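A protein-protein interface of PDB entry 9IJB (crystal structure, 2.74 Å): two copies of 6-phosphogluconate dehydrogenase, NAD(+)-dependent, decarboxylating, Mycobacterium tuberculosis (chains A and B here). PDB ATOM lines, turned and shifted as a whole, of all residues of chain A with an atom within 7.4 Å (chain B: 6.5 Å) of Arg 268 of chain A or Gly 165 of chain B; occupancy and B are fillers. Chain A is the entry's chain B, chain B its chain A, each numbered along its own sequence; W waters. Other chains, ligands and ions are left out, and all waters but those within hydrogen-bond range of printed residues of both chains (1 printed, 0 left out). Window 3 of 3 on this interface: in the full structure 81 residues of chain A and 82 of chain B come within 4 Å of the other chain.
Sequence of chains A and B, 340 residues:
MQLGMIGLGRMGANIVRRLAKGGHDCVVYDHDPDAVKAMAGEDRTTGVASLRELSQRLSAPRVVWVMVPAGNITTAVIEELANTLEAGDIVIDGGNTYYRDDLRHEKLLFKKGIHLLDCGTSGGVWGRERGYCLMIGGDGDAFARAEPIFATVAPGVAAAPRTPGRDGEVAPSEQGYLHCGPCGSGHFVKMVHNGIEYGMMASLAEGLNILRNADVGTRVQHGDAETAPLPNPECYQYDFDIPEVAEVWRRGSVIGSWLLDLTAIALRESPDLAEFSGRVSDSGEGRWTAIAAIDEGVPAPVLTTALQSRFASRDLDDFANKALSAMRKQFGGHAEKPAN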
ATOM      1  N   PRO A 243      32.064 -23.925  -2.855  1.00  0.00           N
ATOM      2  CA  PRO A 243      31.202 -25.068  -2.505  1.00  0.00           C
ATOM      3  C   PRO A 243      31.971 -26.306  -2.095  1.00  0.00           C
ATOM      4  O   PRO A 243      31.537 -27.047  -1.204  1.00  0.00           O
ATOM      5  CB  PRO A 243      30.397 -25.287  -3.790  1.00  0.00           C
ATOM      6  CG  PRO A 243      30.188 -23.900  -4.299  1.00  0.00           C
ATOM      7  CD  PRO A 243      31.538 -23.226  -4.045  1.00  0.00           C
ATOM      8  N   GLU A 244      33.129 -26.525  -2.711  1.00  0.00           N
ATOM      9  CA  GLU A 244      33.968 -27.685  -2.429  1.00  0.00           C
ATOM     10  C   GLU A 244      34.754 -27.538  -1.127  1.00  0.00           C
ATOM     11  O   GLU A 244      34.827 -28.488  -0.336  1.00  0.00           O
ATOM     12  CB  GLU A 244      34.916 -27.917  -3.607  1.00  0.00           C
ATOM     13  CG  GLU A 244      34.185 -28.353  -4.851  1.00  0.00           C
ATOM     14  CD  GLU A 244      33.141 -29.420  -4.552  1.00  0.00           C
ATOM     15  OE1 GLU A 244      31.957 -29.060  -4.357  1.00  0.00           O
ATOM     16  OE2 GLU A 244      33.509 -30.618  -4.525  1.00  0.00           O
ATOM     17  N   ALA A 246      33.778 -25.860   1.399  1.00  0.00           N
ATOM     18  CA  ALA A 246      32.834 -25.976   2.504  1.00  0.00           C
ATOM     19  C   ALA A 246      32.558 -27.432   2.830  1.00  0.00           C
ATOM     20  O   ALA A 246      32.422 -27.789   4.007  1.00  0.00           O
ATOM     21  CB  ALA A 246      31.529 -25.248   2.182  1.00  0.00           C
ATOM     22  N   GLU A 247      32.511 -28.294   1.796  1.00  0.00           N
ATOM     23  CA  GLU A 247      32.213 -29.687   2.113  1.00  0.00           C
ATOM     24  C   GLU A 247      33.490 -30.466   2.465  1.00  0.00           C
ATOM     25  O   GLU A 247      33.442 -31.402   3.265  1.00  0.00           O
ATOM     26  CB  GLU A 247      31.468 -30.363   0.936  1.00  0.00           C
ATOM     27  CG  GLU A 247      31.497 -31.870   0.947  1.00  0.00           C
ATOM     28  CD  GLU A 247      30.234 -32.440   1.604  1.00  0.00           C
ATOM     29  OE1 GLU A 247      29.140 -31.803   1.542  1.00  0.00           O
ATOM     30  OE2 GLU A 247      30.349 -33.564   2.147  1.00  0.00           O
ATOM     31  N   LEU A 262      25.072 -26.878   6.972  1.00  0.00           N
ATOM     32  CA  LEU A 262      24.042 -26.108   6.291  1.00  0.00           C
ATOM     33  C   LEU A 262      24.666 -25.175   5.267  1.00  0.00           C
ATOM     34  O   LEU A 262      24.123 -24.993   4.166  1.00  0.00           O
ATOM     35  CB  LEU A 262      23.218 -25.313   7.302  1.00  0.00           C
ATOM     36  CG  LEU A 262      22.612 -26.115   8.454  1.00  0.00           C
ATOM     37  CD1 LEU A 262      21.968 -25.231   9.508  1.00  0.00           C
ATOM     38  CD2 LEU A 262      21.625 -27.172   7.956  1.00  0.00           C
ATOM     39  N   THR A 263      25.806 -24.573   5.610  1.00  0.00           N
ATOM     40  CA  THR A 263      26.499 -23.758   4.621  1.00  0.00           C
ATOM     41  C   THR A 263      26.842 -24.596   3.400  1.00  0.00           C
ATOM     42  O   THR A 263      26.666 -24.148   2.264  1.00  0.00           O
ATOM     43  CB  THR A 263      27.740 -23.104   5.234  1.00  0.00           C
ATOM     44  OG1 THR A 263      27.363 -22.278   6.353  1.00  0.00           O
ATOM     45  CG2 THR A 263      28.465 -22.243   4.221  1.00  0.00           C
ATOM     46  N   ALA A 264      27.243 -25.851   3.619  1.00  0.00           N
ATOM     47  CA  ALA A 264      27.591 -26.735   2.513  1.00  0.00           C
ATOM     48  C   ALA A 264      26.388 -26.975   1.605  1.00  0.00           C
ATOM     49  O   ALA A 264      26.509 -26.928   0.370  1.00  0.00           O
ATOM     50  CB  ALA A 264      28.134 -28.054   3.064  1.00  0.00           C
ATOM     51  N   ILE A 265      25.215 -27.210   2.212  1.00  0.00           N
ATOM     52  CA  ILE A 265      23.985 -27.425   1.455  1.00  0.00           C
ATOM     53  C   ILE A 265      23.705 -26.231   0.554  1.00  0.00           C
ATOM     54  O   ILE A 265      23.464 -26.382  -0.648  1.00  0.00           O
ATOM     55  CB  ILE A 265      22.806 -27.679   2.412  1.00  0.00           C
ATOM     56  CG1 ILE A 265      22.943 -29.032   3.115  1.00  0.00           C
ATOM     57  CG2 ILE A 265      21.428 -27.559   1.680  1.00  0.00           C
ATOM     58  CD1 ILE A 265      21.700 -29.413   3.904  1.00  0.00           C
ATOM     59  N   ALA A 266      23.744 -25.027   1.135  1.00  0.00           N
ATOM     60  CA  ALA A 266      23.345 -23.818   0.424  1.00  0.00           C
ATOM     61  C   ALA A 266      24.270 -23.521  -0.751  1.00  0.00           C
ATOM     62  O   ALA A 266      23.811 -23.067  -1.804  1.00  0.00           O
ATOM     63  CB  ALA A 266      23.326 -22.636   1.394  1.00  0.00           C
ATOM     64  N   LEU A 267      25.580 -23.744  -0.581  1.00  0.00           N
ATOM     65  CA  LEU A 267      26.512 -23.520  -1.686  1.00  0.00           C
ATOM     66  C   LEU A 267      26.321 -24.547  -2.793  1.00  0.00           C
ATOM     67  O   LEU A 267      26.600 -24.259  -3.963  1.00  0.00           O
ATOM     68  CB  LEU A 267      27.960 -23.551  -1.186  1.00  0.00           C
ATOM     69  CG  LEU A 267      28.320 -22.358  -0.286  1.00  0.00           C
ATOM     70  CD1 LEU A 267      29.623 -22.584   0.392  1.00  0.00           C
ATOM     71  CD2 LEU A 267      28.378 -21.066  -1.078  1.00  0.00           C
ATOM     72  N   ARG A 268      25.872 -25.751  -2.441  1.00  0.00           N
ATOM     73  CA  ARG A 268      25.552 -26.758  -3.442  1.00  0.00           C
ATOM     74  C   ARG A 268      24.318 -26.325  -4.243  1.00  0.00           C
ATOM     75  O   ARG A 268      24.275 -26.497  -5.468  1.00  0.00           O
ATOM     76  CB  ARG A 268      25.307 -28.100  -2.747  1.00  0.00           C
ATOM     77  CG  ARG A 268      25.062 -29.302  -3.665  1.00  0.00           C
ATOM     78  CD  ARG A 268      26.288 -29.608  -4.532  1.00  0.00           C
ATOM     79  NE  ARG A 268      26.035 -30.675  -5.506  1.00  0.00           N
ATOM     80  CZ  ARG A 268      26.975 -31.242  -6.260  1.00  0.00           C
ATOM     81  NH1 ARG A 268      28.247 -30.851  -6.169  1.00  0.00           N
ATOM     82  NH2 ARG A 268      26.644 -32.202  -7.107  1.00  0.00           N
ATOM     83  N   GLU A 269      23.314 -25.742  -3.573  1.00  0.00           N
ATOM     84  CA  GLU A 269      22.155 -25.183  -4.274  1.00  0.00           C
ATOM     85  C   GLU A 269      22.520 -23.922  -5.065  1.00  0.00           C
ATOM     86  O   GLU A 269      22.057 -23.739  -6.201  1.00  0.00           O
ATOM     87  CB  GLU A 269      21.030 -24.870  -3.275  1.00  0.00           C
ATOM     88  CG  GLU A 269      20.562 -26.069  -2.468  1.00  0.00           C
ATOM     89  CD  GLU A 269      19.357 -25.741  -1.580  1.00  0.00           C
ATOM     90  OE1 GLU A 269      19.089 -24.536  -1.352  1.00  0.00           O
ATOM     91  OE2 GLU A 269      18.685 -26.691  -1.111  1.00  0.00           O
ATOM     92  N   SER A 270      23.335 -23.042  -4.484  1.00  0.00           N
ATOM     93  CA  SER A 270      23.670 -21.749  -5.079  1.00  0.00           C
ATOM     94  C   SER A 270      25.136 -21.424  -4.848  1.00  0.00           C
ATOM     95  O   SER A 270      25.498 -20.920  -3.772  1.00  0.00           O
ATOM     96  CB  SER A 270      22.797 -20.662  -4.472  1.00  0.00           C
ATOM     97  OG  SER A 270      22.653 -19.585  -5.373  1.00  0.00           O
ATOM     98  N   PRO A 271      26.005 -21.671  -5.831  1.00  0.00           N
ATOM     99  CA  PRO A 271      27.453 -21.496  -5.600  1.00  0.00           C
ATOM    100  C   PRO A 271      27.886 -20.064  -5.402  1.00  0.00           C
ATOM    101  O   PRO A 271      29.043 -19.843  -5.025  1.00  0.00           O
ATOM    102  CB  PRO A 271      28.095 -22.085  -6.861  1.00  0.00           C
ATOM    103  CG  PRO A 271      27.049 -22.953  -7.463  1.00  0.00           C
ATOM    104  CD  PRO A 271      25.715 -22.418  -7.068  1.00  0.00           C
ATOM    105  N   LEU A 273      25.591 -17.869  -3.772  1.00  0.00           N
ATOM    106  CA  LEU A 273      24.550 -17.396  -2.858  1.00  0.00           C
ATOM    107  C   LEU A 273      23.828 -16.185  -3.438  1.00  0.00           C
ATOM    108  O   LEU A 273      23.531 -15.218  -2.735  1.00  0.00           O
ATOM    109  CB  LEU A 273      25.123 -17.083  -1.483  1.00  0.00           C
ATOM    110  CG  LEU A 273      25.967 -18.202  -0.886  1.00  0.00           C
ATOM    111  CD1 LEU A 273      26.619 -17.703   0.395  1.00  0.00           C
ATOM    112  CD2 LEU A 273      25.102 -19.466  -0.650  1.00  0.00           C
ATOM    113  N   ARG B 162      26.076 -37.829   3.627  1.00  0.00           N
ATOM    114  CA  ARG B 162      26.241 -36.977   2.460  1.00  0.00           C
ATOM    115  C   ARG B 162      25.430 -35.697   2.605  1.00  0.00           C
ATOM    116  O   ARG B 162      24.345 -35.684   3.198  1.00  0.00           O
ATOM    117  CB  ARG B 162      25.841 -37.721   1.189  1.00  0.00           C
ATOM    118  CG  ARG B 162      26.813 -38.824   0.794  1.00  0.00           C
ATOM    119  CD  ARG B 162      26.461 -39.420  -0.537  1.00  0.00           C
ATOM    120  NE  ARG B 162      27.131 -38.721  -1.615  1.00  0.00           N
ATOM    121  CZ  ARG B 162      26.818 -38.846  -2.900  1.00  0.00           C
ATOM    122  NH1 ARG B 162      25.843 -39.667  -3.269  1.00  0.00           N
ATOM    123  NH2 ARG B 162      27.485 -38.147  -3.815  1.00  0.00           N
ATOM    124  N   THR B 163      25.980 -34.610   2.092  1.00  0.00           N
ATOM    125  CA  THR B 163      25.189 -33.389   2.124  1.00  0.00           C
ATOM    126  C   THR B 163      23.999 -33.520   1.173  1.00  0.00           C
ATOM    127  O   THR B 163      24.170 -33.966   0.032  1.00  0.00           O
ATOM    128  CB  THR B 163      26.048 -32.192   1.736  1.00  0.00           C
ATOM    129  OG1 THR B 163      27.029 -31.962   2.751  1.00  0.00           O
ATOM    130  CG2 THR B 163      25.195 -30.949   1.597  1.00  0.00           C
ATOM    131  N   PRO B 164      22.826 -33.086   1.634  1.00  0.00           N
ATOM    132  CA  PRO B 164      21.655 -33.081   0.750  1.00  0.00           C
ATOM    133  C   PRO B 164      21.934 -32.237  -0.484  1.00  0.00           C
ATOM    134  O   PRO B 164      22.473 -31.131  -0.396  1.00  0.00           O
ATOM    135  CB  PRO B 164      20.555 -32.469   1.622  1.00  0.00           C
ATOM    136  CG  PRO B 164      21.005 -32.711   3.034  1.00  0.00           C
ATOM    137  CD  PRO B 164      22.502 -32.634   2.998  1.00  0.00           C
ATOM    138  N   GLY B 165      21.569 -32.774  -1.641  1.00  0.00           N
ATOM    139  CA  GLY B 165      21.908 -32.182  -2.915  1.00  0.00           C
ATOM    140  C   GLY B 165      23.126 -32.792  -3.577  1.00  0.00           C
ATOM    141  O   GLY B 165      23.302 -32.630  -4.792  1.00  0.00           O
ATOM    142  N   ARG B 166      23.972 -33.477  -2.805  1.00  0.00           N
ATOM    143  CA  ARG B 166      25.046 -34.281  -3.377  1.00  0.00           C
ATOM    144  C   ARG B 166      24.474 -35.426  -4.200  1.00  0.00           C
ATOM    145  O   ARG B 166      23.633 -36.201  -3.726  1.00  0.00           O
ATOM    146  CB  ARG B 166      25.946 -34.838  -2.283  1.00  0.00           C
ATOM    147  CG  ARG B 166      26.959 -33.850  -1.802  1.00  0.00           C
ATOM    148  CD  ARG B 166      27.827 -33.434  -2.936  1.00  0.00           C
ATOM    149  NE  ARG B 166      28.368 -32.112  -2.671  1.00  0.00           N
ATOM    150  CZ  ARG B 166      29.553 -31.701  -3.097  1.00  0.00           C
ATOM    151  NH1 ARG B 166      30.317 -32.528  -3.803  1.00  0.00           N
ATOM    152  NH2 ARG B 166      29.965 -30.473  -2.808  1.00  0.00           N
ATOM    153  N   ASP B 167      24.962 -35.546  -5.428  1.00  0.00           N
ATOM    154  CA  ASP B 167      24.339 -36.377  -6.441  1.00  0.00           C
ATOM    155  C   ASP B 167      25.257 -37.541  -6.788  1.00  0.00           C
ATOM    156  O   ASP B 167      26.443 -37.338  -7.077  1.00  0.00           O
ATOM    157  CB  ASP B 167      24.016 -35.549  -7.693  1.00  0.00           C
ATOM    158  CG  ASP B 167      22.733 -34.726  -7.542  1.00  0.00           C
ATOM    159  OD1 ASP B 167      21.635 -35.329  -7.511  1.00  0.00           O
ATOM    160  OD2 ASP B 167      22.819 -33.477  -7.456  1.00  0.00           O
ATOM    161  N   ALA B 171      32.311 -37.249  -4.875  1.00  0.00           N
ATOM    162  CA  ALA B 171      33.351 -36.304  -5.241  1.00  0.00           C
ATOM    163  C   ALA B 171      34.445 -36.289  -4.172  1.00  0.00           C
ATOM    164  O   ALA B 171      34.179 -36.581  -3.002  1.00  0.00           O
ATOM    165  CB  ALA B 171      32.757 -34.908  -5.403  1.00  0.00           C
HETATM  166  O   HOH W   1      28.492 -34.992   1.543  1.00  0.00           O
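Water W1 lies within hydrogen-bond range of OE2 of Glu 247 of chain A (2.4 Å) and N of Thr 163 of chain B (2.6 Å).
No position is printed for both chains.
Of the 6 pairs that touch across the chains among the printed residues, none has its exchanged pair printed and touching as well.
Arg 268 of chain A touches just these residues of chain B: Gly 165 (3.4 Å) and Arg 166 (3.4 Å).
Gly 165 of chain B touches just one residue of chain A: Arg 268.
Of the printed residues of chain B, Ile 265 of chain A touches Thr 163 (3.3 Å) and Pro 164 (3.4 Å).
Printed residues of chain B within 4 Å of Glu 247 of chain A: Thr 163 (2.4 Å).
Of the printed residues of chain B, Glu 244 of chain A touches Arg 166 (2.9 Å).
The nearest residue of chain A that does not touch Gly 165 of chain B is Ile 265 of chain A (6.2 Å).
The nearest printed residue of chain A that does not touch Thr 163 of chain B is Ala 264 of chain A (4.1 Å).
The side-chain hydroxyl (OG1) of Thr 163 of chain B lies within hydrogen-bond range of the side-chain carboxylate (OE1) of Glu 247 of chain A (2.4 Å).
O of Gly 165 of chain B lies within hydrogen-bond range of NE of Arg 268 of chain A (3.4 Å).
NH2 of Arg 166 of chain B is in salt-bridge range of OE1 of Glu 244 of chain A, 2.9 Å away.
Of the 15 printed residues of chain A, 4 touch a printed residue of chain B.
Hydrophobic or aromatic side chains of chain A that line the printed part of chain B: Ile 265.
Hydrophobic or aromatic side chains of chain B that line the printed part of chain A: Pro 164.
Among the printed residues, 6 pairs touch across the chains.
Thr 163 of chain B touches Ile 265 of chain A (CG2 to CG1, 3.3 Å).
Pro 164 of chain B touches Ile 265 of chain A (CD to CD1, 3.4 Å).
Arg 268 of chain A touches Arg 166 of chain B (NH1 to CZ, 3.4 Å).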
